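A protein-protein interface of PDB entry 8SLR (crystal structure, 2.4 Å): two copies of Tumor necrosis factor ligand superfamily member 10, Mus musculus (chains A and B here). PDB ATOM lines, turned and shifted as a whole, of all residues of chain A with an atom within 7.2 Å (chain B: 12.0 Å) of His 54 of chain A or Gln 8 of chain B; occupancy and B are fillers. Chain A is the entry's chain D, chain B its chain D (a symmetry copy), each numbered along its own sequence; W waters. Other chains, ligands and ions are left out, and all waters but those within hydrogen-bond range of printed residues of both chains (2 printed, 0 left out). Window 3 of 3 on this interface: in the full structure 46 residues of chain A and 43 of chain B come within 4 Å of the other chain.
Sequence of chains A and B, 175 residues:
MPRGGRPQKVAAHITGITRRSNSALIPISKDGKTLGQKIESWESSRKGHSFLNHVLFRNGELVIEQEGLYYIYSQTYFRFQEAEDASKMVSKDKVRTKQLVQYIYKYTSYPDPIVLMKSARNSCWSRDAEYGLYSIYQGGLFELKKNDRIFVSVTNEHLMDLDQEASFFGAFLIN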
ATOM      1  N   LEU A  52      21.308  23.037   0.518  1.00  0.00           N
ATOM      2  CA  LEU A  52      21.376  24.421   0.072  1.00  0.00           C
ATOM      3  C   LEU A  52      21.023  25.321   1.249  1.00  0.00           C
ATOM      4  O   LEU A  52      19.997  25.102   1.900  1.00  0.00           O
ATOM      5  CB  LEU A  52      20.396  24.690  -1.079  1.00  0.00           C
ATOM      6  CG  LEU A  52      20.497  23.836  -2.343  1.00  0.00           C
ATOM      7  CD1 LEU A  52      19.265  24.040  -3.213  1.00  0.00           C
ATOM      8  CD2 LEU A  52      21.757  24.170  -3.128  1.00  0.00           C
ATOM      9  N   ASN A  53      21.867  26.327   1.503  1.00  0.00           N
ATOM     10  CA  ASN A  53      21.633  27.353   2.522  1.00  0.00           C
ATOM     11  C   ASN A  53      21.843  28.718   1.866  1.00  0.00           C
ATOM     12  O   ASN A  53      22.987  29.135   1.665  1.00  0.00           O
ATOM     13  CB  ASN A  53      22.574  27.191   3.719  1.00  0.00           C
ATOM     14  CG  ASN A  53      22.319  25.922   4.516  1.00  0.00           C
ATOM     15  OD1 ASN A  53      21.253  25.315   4.430  1.00  0.00           O
ATOM     16  ND2 ASN A  53      23.306  25.525   5.310  1.00  0.00           N
ATOM     17  N   HIS A  54      20.752  29.421   1.543  1.00  0.00           N
ATOM     18  CA  HIS A  54      20.836  30.746   0.926  1.00  0.00           C
ATOM     19  C   HIS A  54      21.612  30.712  -0.383  1.00  0.00           C
ATOM     20  O   HIS A  54      22.308  31.667  -0.742  1.00  0.00           O
ATOM     21  CB  HIS A  54      21.436  31.756   1.900  1.00  0.00           C
ATOM     22  CG  HIS A  54      20.747  31.758   3.225  1.00  0.00           C
ATOM     23  ND1 HIS A  54      19.407  32.042   3.359  1.00  0.00           N
ATOM     24  CD2 HIS A  54      21.200  31.467   4.467  1.00  0.00           C
ATOM     25  CE1 HIS A  54      19.066  31.944   4.631  1.00  0.00           C
ATOM     26  NE2 HIS A  54      20.136  31.599   5.323  1.00  0.00           N
ATOM     27  N   VAL A  55      21.498  29.590  -1.083  1.00  0.00           N
ATOM     28  CA  VAL A  55      21.933  29.450  -2.461  1.00  0.00           C
ATOM     29  C   VAL A  55      20.818  28.713  -3.177  1.00  0.00           C
ATOM     30  O   VAL A  55      20.245  27.764  -2.631  1.00  0.00           O
ATOM     31  CB  VAL A  55      23.261  28.686  -2.584  1.00  0.00           C
ATOM     32  CG1 VAL A  55      23.690  28.612  -4.038  1.00  0.00           C
ATOM     33  CG2 VAL A  55      24.340  29.343  -1.735  1.00  0.00           C
ATOM     34  N   LEU A  56      20.486  29.169  -4.378  1.00  0.00           N
ATOM     35  CA  LEU A  56      19.437  28.541  -5.158  1.00  0.00           C
ATOM     36  C   LEU A  56      20.054  27.537  -6.114  1.00  0.00           C
ATOM     37  O   LEU A  56      21.226  27.648  -6.487  1.00  0.00           O
ATOM     38  CB  LEU A  56      18.643  29.583  -5.939  1.00  0.00           C
ATOM     39  CG  LEU A  56      17.918  30.646  -5.115  1.00  0.00           C
ATOM     40  CD1 LEU A  56      17.424  31.758  -6.018  1.00  0.00           C
ATOM     41  CD2 LEU A  56      16.765  30.034  -4.333  1.00  0.00           C
ATOM     42  N   VAL A  63      22.806  29.483  -8.074  1.00  0.00           N
ATOM     43  CA  VAL A  63      22.478  30.877  -8.346  1.00  0.00           C
ATOM     44  C   VAL A  63      22.628  31.657  -7.050  1.00  0.00           C
ATOM     45  O   VAL A  63      22.046  31.289  -6.021  1.00  0.00           O
ATOM     46  CB  VAL A  63      21.062  31.014  -8.937  1.00  0.00           C
ATOM     47  CG1 VAL A  63      20.702  32.476  -9.163  1.00  0.00           C
ATOM     48  CG2 VAL A  63      20.965  30.224 -10.243  1.00  0.00           C
ATOM     49  N   ILE A  64      23.392  32.735  -7.111  1.00  0.00           N
ATOM     50  CA  ILE A  64      23.849  33.431  -5.917  1.00  0.00           C
ATOM     51  C   ILE A  64      22.737  34.336  -5.406  1.00  0.00           C
ATOM     52  O   ILE A  64      22.143  35.113  -6.168  1.00  0.00           O
ATOM     53  CB  ILE A  64      25.128  34.231  -6.222  1.00  0.00           C
ATOM     54  CG1 ILE A  64      26.241  33.304  -6.755  1.00  0.00           C
ATOM     55  CG2 ILE A  64      25.606  35.000  -4.986  1.00  0.00           C
ATOM     56  CD1 ILE A  64      26.618  32.135  -5.834  1.00  0.00           C
ATOM     57  N   GLU A  65      22.457  34.239  -4.110  1.00  0.00           N
ATOM     58  CA  GLU A  65      21.536  35.141  -3.432  1.00  0.00           C
ATOM     59  C   GLU A  65      22.241  36.288  -2.727  1.00  0.00           C
ATOM     60  O   GLU A  65      21.660  37.370  -2.606  1.00  0.00           O
ATOM     61  CB  GLU A  65      20.705  34.379  -2.398  1.00  0.00           C
ATOM     62  CG  GLU A  65      19.820  33.286  -2.972  1.00  0.00           C
ATOM     63  CD  GLU A  65      19.058  32.534  -1.887  1.00  0.00           C
ATOM     64  OE1 GLU A  65      18.669  33.159  -0.879  1.00  0.00           O
ATOM     65  OE2 GLU A  65      18.866  31.313  -2.030  1.00  0.00           O
ATOM     66  N   GLN A  66      23.478  36.078  -2.274  1.00  0.00           N
ATOM     67  CA  GLN A  66      24.212  37.038  -1.452  1.00  0.00           C
ATOM     68  C   GLN A  66      25.550  37.337  -2.118  1.00  0.00           C
ATOM     69  O   GLN A  66      26.401  36.449  -2.227  1.00  0.00           O
ATOM     70  CB  GLN A  66      24.409  36.479  -0.035  1.00  0.00           C
ATOM     71  CG  GLN A  66      25.326  37.272   0.899  1.00  0.00           C
ATOM     72  CD  GLN A  66      24.838  38.679   1.159  1.00  0.00           C
ATOM     73  OE1 GLN A  66      23.723  38.879   1.640  1.00  0.00           O
ATOM     74  NE2 GLN A  66      25.676  39.668   0.844  1.00  0.00           N
ATOM     75  N   TYR A  70      33.249  33.706  -2.656  1.00  0.00           N
ATOM     76  CA  TYR A  70      32.908  32.298  -2.513  1.00  0.00           C
ATOM     77  C   TYR A  70      34.111  31.445  -2.877  1.00  0.00           C
ATOM     78  O   TYR A  70      34.817  31.738  -3.849  1.00  0.00           O
ATOM     79  CB  TYR A  70      31.725  31.907  -3.412  1.00  0.00           C
ATOM     80  CG  TYR A  70      30.382  32.439  -2.965  1.00  0.00           C
ATOM     81  CD1 TYR A  70      30.040  33.769  -3.167  1.00  0.00           C
ATOM     82  CD2 TYR A  70      29.450  31.608  -2.354  1.00  0.00           C
ATOM     83  CE1 TYR A  70      28.813  34.260  -2.770  1.00  0.00           C
ATOM     84  CE2 TYR A  70      28.221  32.092  -1.949  1.00  0.00           C
ATOM     85  CZ  TYR A  70      27.908  33.418  -2.162  1.00  0.00           C
ATOM     86  OH  TYR A  70      26.680  33.904  -1.766  1.00  0.00           O
ATOM     87  N   LEU A 173      30.236  30.870   1.110  1.00  0.00           N
ATOM     88  CA  LEU A 173      30.582  32.273   1.265  1.00  0.00           C
ATOM     89  C   LEU A 173      31.614  32.439   2.372  1.00  0.00           C
ATOM     90  O   LEU A 173      31.493  31.851   3.451  1.00  0.00           O
ATOM     91  CB  LEU A 173      29.326  33.086   1.598  1.00  0.00           C
ATOM     92  CG  LEU A 173      29.440  34.594   1.857  1.00  0.00           C
ATOM     93  CD1 LEU A 173      29.699  35.337   0.572  1.00  0.00           C
ATOM     94  CD2 LEU A 173      28.171  35.112   2.500  1.00  0.00           C
ATOM     95  N   ASN A 175      33.126  34.921   5.004  1.00  0.00           N
ATOM     96  CA  ASN A 175      32.878  36.146   5.751  1.00  0.00           C
ATOM     97  C   ASN A 175      34.190  36.714   6.292  1.00  0.00           C
ATOM     98  O   ASN A 175      35.084  35.978   6.732  1.00  0.00           O
ATOM     99  CB  ASN A 175      31.892  35.878   6.890  1.00  0.00           C
ATOM    100  CG  ASN A 175      30.549  35.378   6.387  1.00  0.00           C
ATOM    101  OD1 ASN A 175      29.765  36.140   5.817  1.00  0.00           O
ATOM    102  ND2 ASN A 175      30.278  34.092   6.594  1.00  0.00           N
ATOM    103  OXT ASN A 175      34.389  37.930   6.294  1.00  0.00           O
ATOM    104  N   GLN B   8      25.420  34.754   8.984  1.00  0.00           N
ATOM    105  CA  GLN B   8      24.660  33.626   8.447  1.00  0.00           C
ATOM    106  C   GLN B   8      25.513  32.797   7.499  1.00  0.00           C
ATOM    107  O   GLN B   8      26.262  33.351   6.688  1.00  0.00           O
ATOM    108  CB  GLN B   8      23.406  34.114   7.718  1.00  0.00           C
ATOM    109  CG  GLN B   8      23.666  35.152   6.637  1.00  0.00           C
ATOM    110  CD  GLN B   8      22.399  35.545   5.884  1.00  0.00           C
ATOM    111  OE1 GLN B   8      21.526  34.713   5.640  1.00  0.00           O
ATOM    112  NE2 GLN B   8      22.296  36.821   5.517  1.00  0.00           N
ATOM    113  N   LYS B   9      25.400  31.471   7.590  1.00  0.00           N
ATOM    114  CA  LYS B   9      26.188  30.596   6.735  1.00  0.00           C
ATOM    115  C   LYS B   9      25.474  30.447   5.402  1.00  0.00           C
ATOM    116  O   LYS B   9      24.267  30.185   5.353  1.00  0.00           O
ATOM    117  CB  LYS B   9      26.450  29.231   7.381  1.00  0.00           C
ATOM    118  CG  LYS B   9      25.256  28.348   7.681  1.00  0.00           C
ATOM    119  CD  LYS B   9      25.750  26.930   7.985  1.00  0.00           C
ATOM    120  CE  LYS B   9      24.745  26.079   8.758  1.00  0.00           C
ATOM    121  NZ  LYS B   9      25.454  25.154   9.698  1.00  0.00           N
ATOM    122  N   VAL B  10      26.220  30.671   4.329  1.00  0.00           N
ATOM    123  CA  VAL B  10      25.724  30.629   2.968  1.00  0.00           C
ATOM    124  C   VAL B  10      26.585  29.611   2.250  1.00  0.00           C
ATOM    125  O   VAL B  10      27.802  29.798   2.134  1.00  0.00           O
ATOM    126  CB  VAL B  10      25.796  32.010   2.296  1.00  0.00           C
ATOM    127  CG1 VAL B  10      25.287  31.952   0.848  1.00  0.00           C
ATOM    128  CG2 VAL B  10      25.009  33.040   3.119  1.00  0.00           C
ATOM    129  N   ALA B  11      25.973  28.519   1.808  1.00  0.00           N
ATOM    130  CA  ALA B  11      26.756  27.430   1.245  1.00  0.00           C
ATOM    131  C   ALA B  11      25.831  26.453   0.538  1.00  0.00           C
ATOM    132  O   ALA B  11      24.611  26.468   0.725  1.00  0.00           O
ATOM    133  CB  ALA B  11      27.565  26.717   2.329  1.00  0.00           C
ATOM    134  N   ALA B  12      26.442  25.585  -0.263  1.00  0.00           N
ATOM    135  CA  ALA B  12      25.721  24.577  -1.017  1.00  0.00           C
ATOM    136  C   ALA B  12      26.672  23.432  -1.320  1.00  0.00           C
ATOM    137  O   ALA B  12      27.864  23.650  -1.552  1.00  0.00           O
ATOM    138  CB  ALA B  12      25.153  25.156  -2.315  1.00  0.00           C
ATOM    139  N   HIS B  13      26.135  22.213  -1.302  1.00  0.00           N
ATOM    140  CA  HIS B  13      26.841  21.036  -1.799  1.00  0.00           C
ATOM    141  C   HIS B  13      25.805  20.136  -2.454  1.00  0.00           C
ATOM    142  O   HIS B  13      24.885  19.669  -1.778  1.00  0.00           O
ATOM    143  CB  HIS B  13      27.567  20.301  -0.667  1.00  0.00           C
ATOM    144  CG  HIS B  13      28.257  19.038  -1.093  1.00  0.00           C
ATOM    145  ND1 HIS B  13      29.571  19.004  -1.515  1.00  0.00           N
ATOM    146  CD2 HIS B  13      27.819  17.758  -1.139  1.00  0.00           C
ATOM    147  CE1 HIS B  13      29.906  17.761  -1.811  1.00  0.00           C
ATOM    148  NE2 HIS B  13      28.860  16.984  -1.594  1.00  0.00           N
ATOM    149  N   ILE B  14      25.933  19.924  -3.759  1.00  0.00           N
ATOM    150  CA  ILE B  14      25.016  19.082  -4.514  1.00  0.00           C
ATOM    151  C   ILE B  14      25.822  17.964  -5.165  1.00  0.00           C
ATOM    152  O   ILE B  14      27.008  18.126  -5.469  1.00  0.00           O
ATOM    153  CB  ILE B  14      24.216  19.913  -5.541  1.00  0.00           C
ATOM    154  CG1 ILE B  14      25.090  20.434  -6.694  1.00  0.00           C
ATOM    155  CG2 ILE B  14      23.577  21.092  -4.827  1.00  0.00           C
ATOM    156  CD1 ILE B  14      24.351  21.401  -7.647  1.00  0.00           C
ATOM    157  N   GLY B  68      27.858  21.271  13.063  1.00  0.00           N
ATOM    158  CA  GLY B  68      27.815  22.320  12.067  1.00  0.00           C
ATOM    159  C   GLY B  68      28.290  21.823  10.715  1.00  0.00           C
ATOM    160  O   GLY B  68      28.448  20.626  10.485  1.00  0.00           O
ATOM    161  N   LEU B  69      28.500  22.787   9.824  1.00  0.00           N
ATOM    162  CA  LEU B  69      28.939  22.519   8.465  1.00  0.00           C
ATOM    163  C   LEU B  69      30.457  22.566   8.413  1.00  0.00           C
ATOM    164  O   LEU B  69      31.065  23.544   8.855  1.00  0.00           O
ATOM    165  CB  LEU B  69      28.341  23.547   7.501  1.00  0.00           C
ATOM    166  CG  LEU B  69      28.704  23.429   6.024  1.00  0.00           C
ATOM    167  CD1 LEU B  69      28.135  22.164   5.436  1.00  0.00           C
ATOM    168  CD2 LEU B  69      28.199  24.645   5.268  1.00  0.00           C
ATOM    169  N   LEU B 141      31.867  19.825   1.347  1.00  0.00           N
ATOM    170  CA  LEU B 141      31.103  20.401   2.445  1.00  0.00           C
ATOM    171  C   LEU B 141      30.067  19.399   2.929  1.00  0.00           C
ATOM    172  O   LEU B 141      29.283  18.880   2.127  1.00  0.00           O
ATOM    173  CB  LEU B 141      30.380  21.666   1.992  1.00  0.00           C
ATOM    174  CG  LEU B 141      31.189  22.888   1.607  1.00  0.00           C
ATOM    175  CD1 LEU B 141      30.298  23.915   0.923  1.00  0.00           C
ATOM    176  CD2 LEU B 141      31.788  23.460   2.856  1.00  0.00           C
ATOM    177  N   GLU B 143      27.395  18.444   6.455  1.00  0.00           N
ATOM    178  CA  GLU B 143      26.825  18.781   7.749  1.00  0.00           C
ATOM    179  C   GLU B 143      27.094  17.636   8.715  1.00  0.00           C
ATOM    180  O   GLU B 143      26.716  16.489   8.446  1.00  0.00           O
ATOM    181  CB  GLU B 143      25.326  19.044   7.619  1.00  0.00           C
ATOM    182  CG  GLU B 143      25.000  20.204   6.688  1.00  0.00           C
ATOM    183  CD  GLU B 143      23.520  20.529   6.619  1.00  0.00           C
ATOM    184  OE1 GLU B 143      22.737  19.693   6.114  1.00  0.00           O
ATOM    185  OE2 GLU B 143      23.139  21.631   7.065  1.00  0.00           O
ATOM    186  N   LEU B 173      35.285  24.171  10.400  1.00  0.00           N
ATOM    187  CA  LEU B 173      33.894  24.565  10.552  1.00  0.00           C
ATOM    188  C   LEU B 173      33.641  25.881   9.830  1.00  0.00           C
ATOM    189  O   LEU B 173      34.425  26.829   9.936  1.00  0.00           O
ATOM    190  CB  LEU B 173      33.555  24.714  12.039  1.00  0.00           C
ATOM    191  CG  LEU B 173      32.151  25.173  12.459  1.00  0.00           C
ATOM    192  CD1 LEU B 173      31.144  24.074  12.239  1.00  0.00           C
ATOM    193  CD2 LEU B 173      32.148  25.582  13.916  1.00  0.00           C
ATOM    194  N   ILE B 174      32.517  25.946   9.127  1.00  0.00           N
ATOM    195  CA  ILE B 174      32.110  27.141   8.402  1.00  0.00           C
ATOM    196  C   ILE B 174      31.035  27.851   9.209  1.00  0.00           C
ATOM    197  O   ILE B 174      29.942  27.310   9.420  1.00  0.00           O
ATOM    198  CB  ILE B 174      31.622  26.788   6.991  1.00  0.00           C
ATOM    199  CG1 ILE B 174      32.844  26.415   6.158  1.00  0.00           C
ATOM    200  CG2 ILE B 174      30.847  27.961   6.366  1.00  0.00           C
ATOM    201  CD1 ILE B 174      32.536  25.661   4.986  1.00  0.00           C
ATOM    202  N   ASN B 175      31.350  29.059   9.657  1.00  0.00           N
ATOM    203  CA  ASN B 175      30.407  29.876  10.405  1.00  0.00           C
ATOM    204  C   ASN B 175      29.592  30.754   9.455  1.00  0.00           C
ATOM    205  O   ASN B 175      30.104  31.284   8.460  1.00  0.00           O
ATOM    206  CB  ASN B 175      31.151  30.734  11.431  1.00  0.00           C
ATOM    207  CG  ASN B 175      31.919  29.896  12.439  1.00  0.00           C
ATOM    208  OD1 ASN B 175      31.325  29.266  13.317  1.00  0.00           O
ATOM    209  ND2 ASN B 175      33.242  29.882  12.316  1.00  0.00           N
ATOM    210  OXT ASN B 175      28.392  30.945   9.659  1.00  0.00           O
HETATM  211  O   HOH W   1      29.139  30.811   4.713  1.00  0.00           O
HETATM  212  O   HOH W   2      21.024  22.968   5.797  1.00  0.00           O
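Water W2 bridges OD1 of Asn 53 of chain A and OE2 of Glu 143 of chain B. Water W1 bridges the backbone carbonyl oxygen of Leu 173 of chain A (2.9 Å) and the backbone NH of Val 10 of chain B (2.9 Å).
Asn 175 of chain A touches its own counterpart, Asn 175 of chain B.
OH of Tyr 70 of chain A lies within hydrogen-bond range of O of Gln 66 of chain A, 2.6 Å away. The backbone NH (N) of Val 55 of chain A is in hydrogen-bond range of the side-chain carboxylate (OE2) of Glu 65 of chain A, at 3.3 Å.
N of Asn 53 of chain A is in hydrogen-bond range of O of Ala 11 of chain B (2.9 Å). A ring nitrogen (NE2) of His 54 of chain A is in hydrogen-bond range of the side-chain amide oxygen (OE1) of Gln 8 of chain B (3.4 Å). O of Asn 175 of chain B is in hydrogen-bond range of ND2 of Asn 175 of chain A (3.4 Å). The backbone NH (N) of Leu 173 of chain A sits at hydrogen-bond distance from the backbone carbonyl oxygen (O) of Val 10 of chain B (2.8 Å).
Hydrophobic or aromatic side chains of chain A within 4 Å of the printed part of chain B: Leu 52, His 54, Val 55, Tyr 70 and Leu 173. Of the 14 printed residues of chain B, 7 touch a printed residue of chain A.
Of the printed residues of chain B, His 54 of chain A touches Gln 8, Lys 9 and Val 10. Of the printed residues of chain B, Val 55 of chain A touches Val 10 and Ala 11. No residue of chain B comes within 4 Å of Leu 56 of chain A. No residue of chain B comes within 4 Å of Glu 65 of chain A. Of the printed residues of chain B, Asn 175 of chain A touches Asn 175 (3.4 Å). Of the printed residues of chain A, Gln 8 of chain B touches His 54. Glu 143 of chain B touches none of the printed residues of chain A. Ile 174 of chain B touches none of the printed residues of chain A. The nearest residue of chain B that does not touch His 54 of chain A is Ala 11 of chain B (4.9 Å).
Among the printed residues, merely in contact across the chains: Leu 52 of chain A with Ala 11 of chain B (3.8 Å), Leu 52 of chain A with Ala 12 of chain B (3.6 Å), Leu 52 of chain A with Ile 14 of chain B (3.96 Å), Asn 53 of chain A with Lys 9 of chain B (3.8 Å), Asn 53 of chain A with Val 10 of chain B (3.4 Å), His 54 of chain A with Lys 9 of chain B (3.4 Å), His 54 of chain A with Val 10 of chain B (3.4 Å), Val 55 of chain A with Val 10 of chain B (3.8 Å), Val 55 of chain A with Ala 11 of chain B (3.8 Å) and Tyr 70 of chain A with Val 10 of chain B (3.5 Å).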
